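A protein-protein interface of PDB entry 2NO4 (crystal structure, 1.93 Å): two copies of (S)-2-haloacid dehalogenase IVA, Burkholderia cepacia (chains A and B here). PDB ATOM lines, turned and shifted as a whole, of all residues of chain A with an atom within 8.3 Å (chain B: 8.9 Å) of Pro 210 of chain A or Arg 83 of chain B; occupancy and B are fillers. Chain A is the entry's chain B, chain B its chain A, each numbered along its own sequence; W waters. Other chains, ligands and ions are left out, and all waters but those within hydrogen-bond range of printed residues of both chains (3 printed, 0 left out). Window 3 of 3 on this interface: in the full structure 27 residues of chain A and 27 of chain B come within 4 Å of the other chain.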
ATOM      1  N   ALA A 188      -9.141  22.516  15.537  1.00  0.00           N
ATOM      2  CA  ALA A 188      -8.680  21.536  14.554  1.00  0.00           C
ATOM      3  C   ALA A 188      -8.196  20.203  15.146  1.00  0.00           C
ATOM      4  O   ALA A 188      -8.424  19.171  14.542  1.00  0.00           O
ATOM      5  CB  ALA A 188      -7.608  22.153  13.612  1.00  0.00           C
ATOM      6  N   ARG A 203     -16.232  21.612  10.906  1.00  0.00           N
ATOM      7  CA  ARG A 203     -15.459  22.728  11.449  1.00  0.00           C
ATOM      8  C   ARG A 203     -16.216  24.068  11.333  1.00  0.00           C
ATOM      9  O   ARG A 203     -16.745  24.394  10.270  1.00  0.00           O
ATOM     10  CB  ARG A 203     -14.135  22.845  10.698  1.00  0.00           C
ATOM     11  CG  ARG A 203     -13.383  24.059  11.170  1.00  0.00           C
ATOM     12  CD  ARG A 203     -11.961  23.925  11.039  1.00  0.00           C
ATOM     13  NE  ARG A 203     -11.281  25.019  11.728  1.00  0.00           N
ATOM     14  CZ  ARG A 203      -9.979  25.237  11.622  1.00  0.00           C
ATOM     15  NH1 ARG A 203      -9.238  24.459  10.849  1.00  0.00           N
ATOM     16  NH2 ARG A 203      -9.424  26.263  12.254  1.00  0.00           N
ATOM     17  N   ASN A 205     -15.022  27.520  11.102  1.00  0.00           N
ATOM     18  CA  ASN A 205     -13.799  28.245  10.797  1.00  0.00           C
ATOM     19  C   ASN A 205     -14.204  29.689  10.540  1.00  0.00           C
ATOM     20  O   ASN A 205     -14.513  30.093   9.407  1.00  0.00           O
ATOM     21  CB  ASN A 205     -13.085  27.597   9.607  1.00  0.00           C
ATOM     22  CG  ASN A 205     -11.660  28.094   9.433  1.00  0.00           C
ATOM     23  OD1 ASN A 205     -11.264  29.134   9.992  1.00  0.00           O
ATOM     24  ND2 ASN A 205     -10.892  27.375   8.633  1.00  0.00           N
ATOM     25  N   GLN A 207     -12.552  32.610  10.871  1.00  0.00           N
ATOM     26  CA  GLN A 207     -11.629  33.535  10.244  1.00  0.00           C
ATOM     27  C   GLN A 207     -10.958  32.956   8.993  1.00  0.00           C
ATOM     28  O   GLN A 207     -10.152  33.584   8.367  1.00  0.00           O
ATOM     29  CB  GLN A 207     -10.568  33.971  11.258  1.00  0.00           C
ATOM     30  CG  GLN A 207     -11.099  34.765  12.456  1.00  0.00           C
ATOM     31  CD  GLN A 207     -10.008  35.040  13.484  1.00  0.00           C
ATOM     32  OE1 GLN A 207      -9.446  36.141  13.526  1.00  0.00           O
ATOM     33  NE2 GLN A 207      -9.691  34.035  14.314  1.00  0.00           N
ATOM     34  N   GLY A 208     -11.335  31.754   8.606  1.00  0.00           N
ATOM     35  CA  GLY A 208     -10.684  31.059   7.472  1.00  0.00           C
ATOM     36  C   GLY A 208      -9.206  30.708   7.728  1.00  0.00           C
ATOM     37  O   GLY A 208      -8.341  30.924   6.876  1.00  0.00           O
ATOM     38  N   ASN A 209      -8.919  30.160   8.905  1.00  0.00           N
ATOM     39  CA  ASN A 209      -7.578  29.657   9.224  1.00  0.00           C
ATOM     40  C   ASN A 209      -7.224  28.494   8.316  1.00  0.00           C
ATOM     41  O   ASN A 209      -8.131  27.815   7.837  1.00  0.00           O
ATOM     42  CB  ASN A 209      -7.527  29.188  10.677  1.00  0.00           C
ATOM     43  CG  ASN A 209      -7.828  30.310  11.663  1.00  0.00           C
ATOM     44  OD1 ASN A 209      -8.456  30.061  12.668  1.00  0.00           O
ATOM     45  ND2 ASN A 209      -7.410  31.534  11.373  1.00  0.00           N
ATOM     46  N   PRO A 210      -5.915  28.256   8.088  1.00  0.00           N
ATOM     47  CA  PRO A 210      -5.451  27.195   7.221  1.00  0.00           C
ATOM     48  C   PRO A 210      -5.867  25.813   7.762  1.00  0.00           C
ATOM     49  O   PRO A 210      -6.149  25.668   8.987  1.00  0.00           O
ATOM     50  CB  PRO A 210      -3.910  27.381   7.220  1.00  0.00           C
ATOM     51  CG  PRO A 210      -3.715  28.780   7.616  1.00  0.00           C
ATOM     52  CD  PRO A 210      -4.772  29.000   8.659  1.00  0.00           C
ATOM     53  N   PRO A 211      -5.969  24.815   6.860  1.00  0.00           N
ATOM     54  CA  PRO A 211      -6.384  23.449   7.242  1.00  0.00           C
ATOM     55  C   PRO A 211      -5.253  22.745   8.060  1.00  0.00           C
ATOM     56  O   PRO A 211      -4.048  23.075   7.889  1.00  0.00           O
ATOM     57  CB  PRO A 211      -6.606  22.761   5.876  1.00  0.00           C
ATOM     58  CG  PRO A 211      -5.615  23.479   4.954  1.00  0.00           C
ATOM     59  CD  PRO A 211      -5.694  24.940   5.410  1.00  0.00           C
ATOM     60  N   GLU A 212      -5.643  21.826   8.955  1.00  0.00           N
ATOM     61  CA  GLU A 212      -4.693  21.011   9.747  1.00  0.00           C
ATOM     62  C   GLU A 212      -5.279  19.607   9.942  1.00  0.00           C
ATOM     63  O   GLU A 212      -6.465  19.427   9.729  1.00  0.00           O
ATOM     64  CB  GLU A 212      -4.450  21.613  11.131  1.00  0.00           C
ATOM     65  CG  GLU A 212      -4.018  23.079  11.173  1.00  0.00           C
ATOM     66  CD  GLU A 212      -3.844  23.567  12.614  1.00  0.00           C
ATOM     67  OE1 GLU A 212      -2.769  23.395  13.205  1.00  0.00           O
ATOM     68  OE2 GLU A 212      -4.775  24.171  13.146  1.00  0.00           O
ATOM     69  N   TYR A 213      -4.454  18.637  10.372  1.00  0.00           N
ATOM     70  CA  TYR A 213      -4.929  17.275  10.697  1.00  0.00           C
ATOM     71  C   TYR A 213      -5.705  16.662   9.530  1.00  0.00           C
ATOM     72  O   TYR A 213      -6.818  16.131   9.680  1.00  0.00           O
ATOM     73  CB  TYR A 213      -5.773  17.280  11.983  1.00  0.00           C
ATOM     74  CG  TYR A 213      -5.029  17.830  13.186  1.00  0.00           C
ATOM     75  CD1 TYR A 213      -5.151  19.179  13.552  1.00  0.00           C
ATOM     76  CD2 TYR A 213      -4.145  16.990  13.923  1.00  0.00           C
ATOM     77  CE1 TYR A 213      -4.451  19.667  14.669  1.00  0.00           C
ATOM     78  CE2 TYR A 213      -3.446  17.470  15.043  1.00  0.00           C
ATOM     79  CZ  TYR A 213      -3.604  18.805  15.401  1.00  0.00           C
ATOM     80  OH  TYR A 213      -2.904  19.251  16.501  1.00  0.00           O
ATOM     81  N   GLU A 214      -5.103  16.741   8.358  1.00  0.00           N
ATOM     82  CA  GLU A 214      -5.770  16.393   7.110  1.00  0.00           C
ATOM     83  C   GLU A 214      -5.978  14.896   6.932  1.00  0.00           C
ATOM     84  O   GLU A 214      -6.834  14.505   6.139  1.00  0.00           O
ATOM     85  CB  GLU A 214      -5.007  16.961   5.923  1.00  0.00           C
ATOM     86  CG  GLU A 214      -4.977  18.488   5.943  1.00  0.00           C
ATOM     87  CD  GLU A 214      -4.801  19.078   4.552  1.00  0.00           C
ATOM     88  OE1 GLU A 214      -5.620  19.948   4.160  1.00  0.00           O
ATOM     89  OE2 GLU A 214      -3.860  18.656   3.846  1.00  0.00           O
ATOM     90  N   LEU A 218     -12.663  16.577   7.093  1.00  0.00           N
ATOM     91  CA  LEU A 218     -13.930  17.115   7.548  1.00  0.00           C
ATOM     92  C   LEU A 218     -15.036  16.686   6.602  1.00  0.00           C
ATOM     93  O   LEU A 218     -14.814  16.532   5.405  1.00  0.00           O
ATOM     94  CB  LEU A 218     -13.866  18.636   7.567  1.00  0.00           C
ATOM     95  CG  LEU A 218     -12.761  19.240   8.443  1.00  0.00           C
ATOM     96  CD1 LEU A 218     -12.654  20.707   8.073  1.00  0.00           C
ATOM     97  CD2 LEU A 218     -13.128  19.067   9.961  1.00  0.00           C
ATOM     98  N   GLN A 221     -17.092  22.285   6.330  1.00  0.00           N
ATOM     99  CA  GLN A 221     -16.594  23.482   7.023  1.00  0.00           C
ATOM    100  C   GLN A 221     -17.518  24.666   6.697  1.00  0.00           C
ATOM    101  O   GLN A 221     -17.896  24.856   5.539  1.00  0.00           O
ATOM    102  CB  GLN A 221     -15.175  23.826   6.566  1.00  0.00           C
ATOM    103  CG  GLN A 221     -14.588  25.089   7.214  1.00  0.00           C
ATOM    104  CD  GLN A 221     -13.111  25.240   6.898  1.00  0.00           C
ATOM    105  OE1 GLN A 221     -12.262  24.973   7.731  1.00  0.00           O
ATOM    106  NE2 GLN A 221     -12.804  25.638   5.686  1.00  0.00           N
ATOM    107  N   LEU B  46       5.981  34.302  13.644  1.00  0.00           N
ATOM    108  CA  LEU B  46       6.013  33.111  12.831  1.00  0.00           C
ATOM    109  C   LEU B  46       6.789  31.971  13.550  1.00  0.00           C
ATOM    110  O   LEU B  46       6.345  30.816  13.584  1.00  0.00           O
ATOM    111  CB  LEU B  46       6.645  33.403  11.460  1.00  0.00           C
ATOM    112  CG  LEU B  46       6.788  32.199  10.510  1.00  0.00           C
ATOM    113  CD1 LEU B  46       5.604  32.153   9.575  1.00  0.00           C
ATOM    114  CD2 LEU B  46       8.082  32.311   9.675  1.00  0.00           C
ATOM    115  N   LEU B  49       4.837  30.543  16.407  1.00  0.00           N
ATOM    116  CA  LEU B  49       3.689  29.742  15.960  1.00  0.00           C
ATOM    117  C   LEU B  49       4.201  28.395  15.407  1.00  0.00           C
ATOM    118  O   LEU B  49       3.608  27.328  15.643  1.00  0.00           O
ATOM    119  CB  LEU B  49       2.850  30.481  14.901  1.00  0.00           C
ATOM    120  CG  LEU B  49       1.651  29.686  14.305  1.00  0.00           C
ATOM    121  CD1 LEU B  49       0.700  29.170  15.379  1.00  0.00           C
ATOM    122  CD2 LEU B  49       0.895  30.518  13.247  1.00  0.00           C
ATOM    123  N   ARG B  53       2.964  24.839  17.151  1.00  0.00           N
ATOM    124  CA  ARG B  53       2.244  23.799  16.326  1.00  0.00           C
ATOM    125  C   ARG B  53       3.029  22.491  16.147  1.00  0.00           C
ATOM    126  O   ARG B  53       2.453  21.414  16.174  1.00  0.00           O
ATOM    127  CB  ARG B  53       1.806  24.327  14.970  1.00  0.00           C
ATOM    128  CG  ARG B  53       0.538  25.180  14.970  1.00  0.00           C
ATOM    129  CD  ARG B  53      -0.631  24.393  15.608  1.00  0.00           C
ATOM    130  NE  ARG B  53      -1.941  24.937  15.220  1.00  0.00           N
ATOM    131  CZ  ARG B  53      -2.514  26.040  15.703  1.00  0.00           C
ATOM    132  NH1 ARG B  53      -3.703  26.369  15.225  1.00  0.00           N
ATOM    133  NH2 ARG B  53      -1.941  26.809  16.651  1.00  0.00           N
ATOM    134  N   TYR B  57       1.325  19.197  17.547  1.00  0.00           N
ATOM    135  CA  TYR B  57       1.094  18.052  16.673  1.00  0.00           C
ATOM    136  C   TYR B  57       1.702  16.796  17.299  1.00  0.00           C
ATOM    137  O   TYR B  57       1.097  15.727  17.208  1.00  0.00           O
ATOM    138  CB  TYR B  57       1.650  18.259  15.257  1.00  0.00           C
ATOM    139  CG  TYR B  57       1.032  19.399  14.431  1.00  0.00           C
ATOM    140  CD1 TYR B  57      -0.258  19.885  14.698  1.00  0.00           C
ATOM    141  CD2 TYR B  57       1.748  19.956  13.367  1.00  0.00           C
ATOM    142  CE1 TYR B  57      -0.821  20.933  13.923  1.00  0.00           C
ATOM    143  CE2 TYR B  57       1.191  21.001  12.567  1.00  0.00           C
ATOM    144  CZ  TYR B  57      -0.082  21.469  12.873  1.00  0.00           C
ATOM    145  OH  TYR B  57      -0.607  22.493  12.140  1.00  0.00           O
ATOM    146  N   ASP B  75       7.547  20.232   9.223  1.00  0.00           N
ATOM    147  CA  ASP B  75       7.097  20.650   7.915  1.00  0.00           C
ATOM    148  C   ASP B  75       5.651  21.141   7.961  1.00  0.00           C
ATOM    149  O   ASP B  75       5.358  22.253   7.517  1.00  0.00           O
ATOM    150  CB  ASP B  75       7.255  19.498   6.908  1.00  0.00           C
ATOM    151  CG  ASP B  75       6.975  19.937   5.476  1.00  0.00           C
ATOM    152  OD1 ASP B  75       5.832  20.248   5.112  1.00  0.00           O
ATOM    153  OD2 ASP B  75       7.909  19.994   4.702  1.00  0.00           O
ATOM    154  N   GLU B  76       4.731  20.315   8.487  1.00  0.00           N
ATOM    155  CA  GLU B  76       3.314  20.719   8.593  1.00  0.00           C
ATOM    156  C   GLU B  76       3.140  21.986   9.420  1.00  0.00           C
ATOM    157  O   GLU B  76       2.355  22.882   9.044  1.00  0.00           O
ATOM    158  CB  GLU B  76       2.454  19.568   9.166  1.00  0.00           C
ATOM    159  CG  GLU B  76       2.354  18.398   8.161  1.00  0.00           C
ATOM    160  CD  GLU B  76       1.824  17.099   8.782  1.00  0.00           C
ATOM    161  OE1 GLU B  76       1.701  17.067  10.023  1.00  0.00           O
ATOM    162  OE2 GLU B  76       1.611  16.109   8.033  1.00  0.00           O
ATOM    163  N   ALA B  77       3.861  22.067  10.545  1.00  0.00           N
ATOM    164  CA  ALA B  77       3.745  23.229  11.407  1.00  0.00           C
ATOM    165  C   ALA B  77       4.241  24.493  10.681  1.00  0.00           C
ATOM    166  O   ALA B  77       3.647  25.546  10.843  1.00  0.00           O
ATOM    167  CB  ALA B  77       4.506  22.999  12.709  1.00  0.00           C
ATOM    168  N   LEU B  78       5.315  24.363   9.899  1.00  0.00           N
ATOM    169  CA  LEU B  78       5.896  25.491   9.177  1.00  0.00           C
ATOM    170  C   LEU B  78       4.923  25.966   8.074  1.00  0.00           C
ATOM    171  O   LEU B  78       4.611  27.170   7.954  1.00  0.00           O
ATOM    172  CB  LEU B  78       7.266  25.126   8.573  1.00  0.00           C
ATOM    173  CG  LEU B  78       7.892  26.261   7.724  1.00  0.00           C
ATOM    174  CD1 LEU B  78       7.972  27.570   8.510  1.00  0.00           C
ATOM    175  CD2 LEU B  78       9.265  25.825   7.209  1.00  0.00           C
ATOM    176  N   THR B  79       4.403  25.017   7.308  1.00  0.00           N
ATOM    177  CA  THR B  79       3.402  25.334   6.306  1.00  0.00           C
ATOM    178  C   THR B  79       2.213  26.092   6.891  1.00  0.00           C
ATOM    179  O   THR B  79       1.754  27.073   6.314  1.00  0.00           O
ATOM    180  CB  THR B  79       2.916  24.044   5.574  1.00  0.00           C
ATOM    181  OG1 THR B  79       4.008  23.515   4.848  1.00  0.00           O
ATOM    182  CG2 THR B  79       1.800  24.332   4.608  1.00  0.00           C
ATOM    183  N   PHE B  80       1.713  25.614   8.025  1.00  0.00           N
ATOM    184  CA  PHE B  80       0.588  26.229   8.714  1.00  0.00           C
ATOM    185  C   PHE B  80       0.918  27.678   9.146  1.00  0.00           C
ATOM    186  O   PHE B  80       0.088  28.576   8.959  1.00  0.00           O
ATOM    187  CB  PHE B  80       0.182  25.423   9.964  1.00  0.00           C
ATOM    188  CG  PHE B  80      -0.925  26.079  10.744  1.00  0.00           C
ATOM    189  CD1 PHE B  80      -2.247  25.961  10.312  1.00  0.00           C
ATOM    190  CD2 PHE B  80      -0.649  26.838  11.886  1.00  0.00           C
ATOM    191  CE1 PHE B  80      -3.303  26.576  11.015  1.00  0.00           C
ATOM    192  CE2 PHE B  80      -1.674  27.476  12.580  1.00  0.00           C
ATOM    193  CZ  PHE B  80      -3.021  27.337  12.141  1.00  0.00           C
ATOM    194  N   ALA B  81       2.092  27.858   9.773  1.00  0.00           N
ATOM    195  CA  ALA B  81       2.581  29.183  10.184  1.00  0.00           C
ATOM    196  C   ALA B  81       2.754  30.189   9.002  1.00  0.00           C
ATOM    197  O   ALA B  81       2.327  31.354   9.119  1.00  0.00           O
ATOM    198  CB  ALA B  81       3.869  29.066  11.076  1.00  0.00           C
ATOM    199  N   LEU B  82       3.386  29.750   7.904  1.00  0.00           N
ATOM    200  CA  LEU B  82       3.557  30.592   6.728  1.00  0.00           C
ATOM    201  C   LEU B  82       2.204  31.001   6.157  1.00  0.00           C
ATOM    202  O   LEU B  82       2.008  32.162   5.789  1.00  0.00           O
ATOM    203  CB  LEU B  82       4.427  29.905   5.646  1.00  0.00           C
ATOM    204  CG  LEU B  82       5.917  29.623   5.979  1.00  0.00           C
ATOM    205  CD1 LEU B  82       6.490  28.593   5.025  1.00  0.00           C
ATOM    206  CD2 LEU B  82       6.772  30.922   5.932  1.00  0.00           C
ATOM    207  N   ARG B  83       1.273  30.047   6.097  1.00  0.00           N
ATOM    208  CA  ARG B  83      -0.095  30.317   5.611  1.00  0.00           C
ATOM    209  C   ARG B  83      -0.821  31.307   6.509  1.00  0.00           C
ATOM    210  O   ARG B  83      -1.452  32.243   6.010  1.00  0.00           O
ATOM    211  CB  ARG B  83      -0.895  29.031   5.451  1.00  0.00           C
ATOM    212  CG  ARG B  83      -0.522  28.261   4.190  1.00  0.00           C
ATOM    213  CD  ARG B  83      -1.228  26.944   4.224  1.00  0.00           C
ATOM    214  NE  ARG B  83      -0.901  26.120   3.079  1.00  0.00           N
ATOM    215  CZ  ARG B  83      -1.277  24.845   2.948  1.00  0.00           C
ATOM    216  NH1 ARG B  83      -1.971  24.216   3.905  1.00  0.00           N
ATOM    217  NH2 ARG B  83      -0.933  24.197   1.856  1.00  0.00           N
ATOM    218  N   THR B  84      -0.691  31.108   7.823  1.00  0.00           N
ATOM    219  CA  THR B  84      -1.284  31.983   8.839  1.00  0.00           C
ATOM    220  C   THR B  84      -0.844  33.454   8.650  1.00  0.00           C
ATOM    221  O   THR B  84      -1.665  34.358   8.788  1.00  0.00           O
ATOM    222  CB  THR B  84      -0.963  31.467  10.278  1.00  0.00           C
ATOM    223  OG1 THR B  84      -1.611  30.190  10.472  1.00  0.00           O
ATOM    224  CG2 THR B  84      -1.454  32.430  11.371  1.00  0.00           C
ATOM    225  N   TYR B  85       0.439  33.654   8.345  1.00  0.00           N
ATOM    226  CA  TYR B  85       1.016  35.004   8.160  1.00  0.00           C
ATOM    227  C   TYR B  85       0.936  35.531   6.721  1.00  0.00           C
ATOM    228  O   TYR B  85       1.426  36.649   6.412  1.00  0.00           O
ATOM    229  CB  TYR B  85       2.437  35.100   8.796  1.00  0.00           C
ATOM    230  CG  TYR B  85       2.295  35.200  10.272  1.00  0.00           C
ATOM    231  CD1 TYR B  85       2.304  34.041  11.062  1.00  0.00           C
ATOM    232  CD2 TYR B  85       2.050  36.444  10.885  1.00  0.00           C
ATOM    233  CE1 TYR B  85       2.091  34.105  12.430  1.00  0.00           C
ATOM    234  CE2 TYR B  85       1.859  36.519  12.241  1.00  0.00           C
ATOM    235  CZ  TYR B  85       1.849  35.333  12.998  1.00  0.00           C
ATOM    236  OH  TYR B  85       1.611  35.370  14.333  1.00  0.00           O
ATOM    237  N   HIS B  86       0.309  34.738   5.856  1.00  0.00           N
ATOM    238  CA  HIS B  86       0.056  35.087   4.432  1.00  0.00           C
ATOM    239  C   HIS B  86       1.344  35.467   3.758  1.00  0.00           C
ATOM    240  O   HIS B  86       1.391  36.441   3.019  1.00  0.00           O
ATOM    241  CB  HIS B  86      -0.896  36.288   4.277  1.00  0.00           C
ATOM    242  CG  HIS B  86      -2.324  35.996   4.596  1.00  0.00           C
ATOM    243  ND1 HIS B  86      -2.722  34.972   5.436  1.00  0.00           N
ATOM    244  CD2 HIS B  86      -3.459  36.632   4.222  1.00  0.00           C
ATOM    245  CE1 HIS B  86      -4.041  34.973   5.536  1.00  0.00           C
ATOM    246  NE2 HIS B  86      -4.509  35.972   4.810  1.00  0.00           N
ATOM    247  N   LEU B  87       2.412  34.745   4.009  1.00  0.00           N
ATOM    248  CA  LEU B  87       3.666  35.310   3.551  1.00  0.00           C
ATOM    249  C   LEU B  87       3.806  35.314   2.004  1.00  0.00           C
ATOM    250  O   LEU B  87       3.203  34.482   1.293  1.00  0.00           O
ATOM    251  CB  LEU B  87       4.857  34.701   4.302  1.00  0.00           C
ATOM    252  CG  LEU B  87       4.963  35.405   5.656  1.00  0.00           C
ATOM    253  CD1 LEU B  87       5.831  34.645   6.596  1.00  0.00           C
ATOM    254  CD2 LEU B  87       5.512  36.819   5.482  1.00  0.00           C
ATOM    255  N   GLU B  88       4.557  36.295   1.489  1.00  0.00           N
ATOM    256  CA  GLU B  88       5.025  36.245   0.105  1.00  0.00           C
ATOM    257  C   GLU B  88       6.108  35.151  -0.049  1.00  0.00           C
ATOM    258  O   GLU B  88       6.968  34.989   0.834  1.00  0.00           O
ATOM    259  CB  GLU B  88       5.588  37.595  -0.317  1.00  0.00           C
ATOM    260  CG  GLU B  88       6.099  37.607  -1.762  1.00  0.00           C
ATOM    261  CD  GLU B  88       6.695  38.934  -2.178  1.00  0.00           C
ATOM    262  OE1 GLU B  88       6.855  39.128  -3.405  1.00  0.00           O
ATOM    263  OE2 GLU B  88       6.994  39.780  -1.299  1.00  0.00           O
ATOM    264  N   ARG B  90       5.980  31.780  -0.047  1.00  0.00           N
ATOM    265  CA  ARG B  90       5.877  30.672   0.911  1.00  0.00           C
ATOM    266  C   ARG B  90       6.874  29.536   0.532  1.00  0.00           C
ATOM    267  O   ARG B  90       7.538  28.968   1.392  1.00  0.00           O
ATOM    268  CB  ARG B  90       4.396  30.200   1.047  1.00  0.00           C
ATOM    269  CG  ARG B  90       3.483  31.108   1.950  1.00  0.00           C
ATOM    270  CD  ARG B  90       2.208  30.376   2.346  1.00  0.00           C
ATOM    271  NE  ARG B  90       1.161  30.459   1.339  1.00  0.00           N
ATOM    272  CZ  ARG B  90       0.286  31.462   1.277  1.00  0.00           C
ATOM    273  NH1 ARG B  90       0.335  32.451   2.156  1.00  0.00           N
ATOM    274  NH2 ARG B  90      -0.634  31.493   0.347  1.00  0.00           N
ATOM    275  N   LEU B  93      10.779  30.499   0.706  1.00  0.00           N
ATOM    276  CA  LEU B  93      10.877  30.707   2.123  1.00  0.00           C
ATOM    277  C   LEU B  93      10.829  29.382   2.924  1.00  0.00           C
ATOM    278  O   LEU B  93      11.652  29.156   3.852  1.00  0.00           O
ATOM    279  CB  LEU B  93       9.765  31.641   2.511  1.00  0.00           C
ATOM    280  CG  LEU B  93       9.902  32.463   3.751  1.00  0.00           C
ATOM    281  CD1 LEU B  93      11.274  33.129   3.800  1.00  0.00           C
ATOM    282  CD2 LEU B  93       8.778  33.481   3.764  1.00  0.00           C
ATOM    283  N   LYS B  94       9.905  28.507   2.534  1.00  0.00           N
ATOM    284  CA  LYS B  94       9.732  27.219   3.225  1.00  0.00           C
ATOM    285  C   LYS B  94      10.986  26.357   3.069  1.00  0.00           C
ATOM    286  O   LYS B  94      11.489  25.836   4.068  1.00  0.00           O
ATOM    287  CB  LYS B  94       8.488  26.455   2.743  1.00  0.00           C
ATOM    288  CG  LYS B  94       8.220  25.212   3.567  1.00  0.00           C
ATOM    289  CD  LYS B  94       6.985  24.516   3.093  1.00  0.00           C
ATOM    290  CE  LYS B  94       6.986  23.121   3.588  1.00  0.00           C
ATOM    291  NZ  LYS B  94       5.881  22.308   3.005  1.00  0.00           N
HETATM  292  O   HOH W   1      -2.859  21.485   2.718  1.00  0.00           O
HETATM  293  O   HOH W   2      -1.957  24.323   6.754  1.00  0.00           O
HETATM  294  O   HOH W   3      -4.226  30.335  11.849  1.00  0.00           O
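The side-chain hydroxyl (OH) of Tyr 57 of chain B sits at hydrogen-bond distance from the side-chain carboxylate (OE1) of Glu 212 of chain A, 2.6 Å away. The guanidinium group (NE) of Arg 53 of chain B lies within salt-bridge range of the side-chain carboxylate (OE1) of Glu 212 of chain A (2.7 Å).
The backbone carbonyl oxygen (O) of Phe 80 of chain B sits at hydrogen-bond distance from the side-chain hydroxyl (OG1) of Thr 84 of chain B (2.8 Å). A ring nitrogen (ND1) of His 86 of chain B sits at hydrogen-bond distance from the backbone carbonyl oxygen (O) of Arg 83 of chain B, at 3.1 Å.
Among the printed residues, merely in contact across the chains: Tyr 213 of chain A with Tyr 57 of chain B (3.3 Å), Glu 212 of chain A with Phe 80 of chain B (3.5 Å), Pro 210 of chain A with Arg 83 of chain B (3.6 Å), Pro 210 of chain A with Phe 80 of chain B (3.6 Å), Pro 210 of chain A with Thr 84 of chain B (3.8 Å) and Pro 211 of chain A with Arg 83 of chain B (3.9 Å).
Of chain B, only Phe 80, Arg 83 and Thr 84 come within 4 Å of Pro 210 of chain A. Of chain A, only Pro 210 and Pro 211 come within 4 Å of Arg 83 of chain B. Of the printed residues of chain B, Pro 211 of chain A touches Arg 83. Printed residues of chain B within 4 Å of Glu 212 of chain A: Arg 53 (2.7 Å), Tyr 57 (2.6 Å) and Phe 80 (3.5 Å). Of the printed residues of chain B, Tyr 213 of chain A touches Tyr 57. Printed residues of chain A within 4 Å of Phe 80 of chain B: Pro 210 and Glu 212. Printed residues of chain A within 4 Å of Arg 53 of chain B: Glu 212 (2.7 Å). Printed residues of chain A within 4 Å of Tyr 57 of chain B: Glu 212 (2.6 Å) and Tyr 213 (3.3 Å). Ala 81 of chain B touches none of the printed residues of chain A. The nearest residue of chain B that does not touch Pro 210 of chain A is Thr 79 of chain B (5.7 Å). The nearest residue of chain A that does not touch Arg 83 of chain B is Glu 214 of chain A (5.6 Å).
Along chain A the printed residues that touch a printed residue of chain B span positions 210 to 213. Of the 21 printed residues of chain B, 5 touch a printed residue of chain A. Printed residues of chain B that touch a printed residue of chain A: Arg 53, Tyr 57, Phe 80, Arg 83 and Thr 84. Among the printed residues, Asp or Glu carboxylates within 4 Å of a Lys or Arg side-chain nitrogen of the other chain: Glu 212 of chain A with Arg 53 of chain B (2.7 Å).
No position is printed for both chains. Of the 8 pairs that touch across the chains among the printed residues, none has its exchanged pair printed and touching as well.
Water W2 bridges O of Pro 211 of chain A (2.7 Å) and NH1 of Arg 83 of chain B (2.9 Å). Water W3 bridges OG1 of Thr 84 of chain B (3.0 Å) and ND2 of Asn 209 of chain A (3.4 Å). Water W1 lies within hydrogen-bond range of the guanidinium group of Arg 83 of chain B (3.1 Å) and the side-chain carboxylate of Glu 214 of chain A (3.2 Å).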
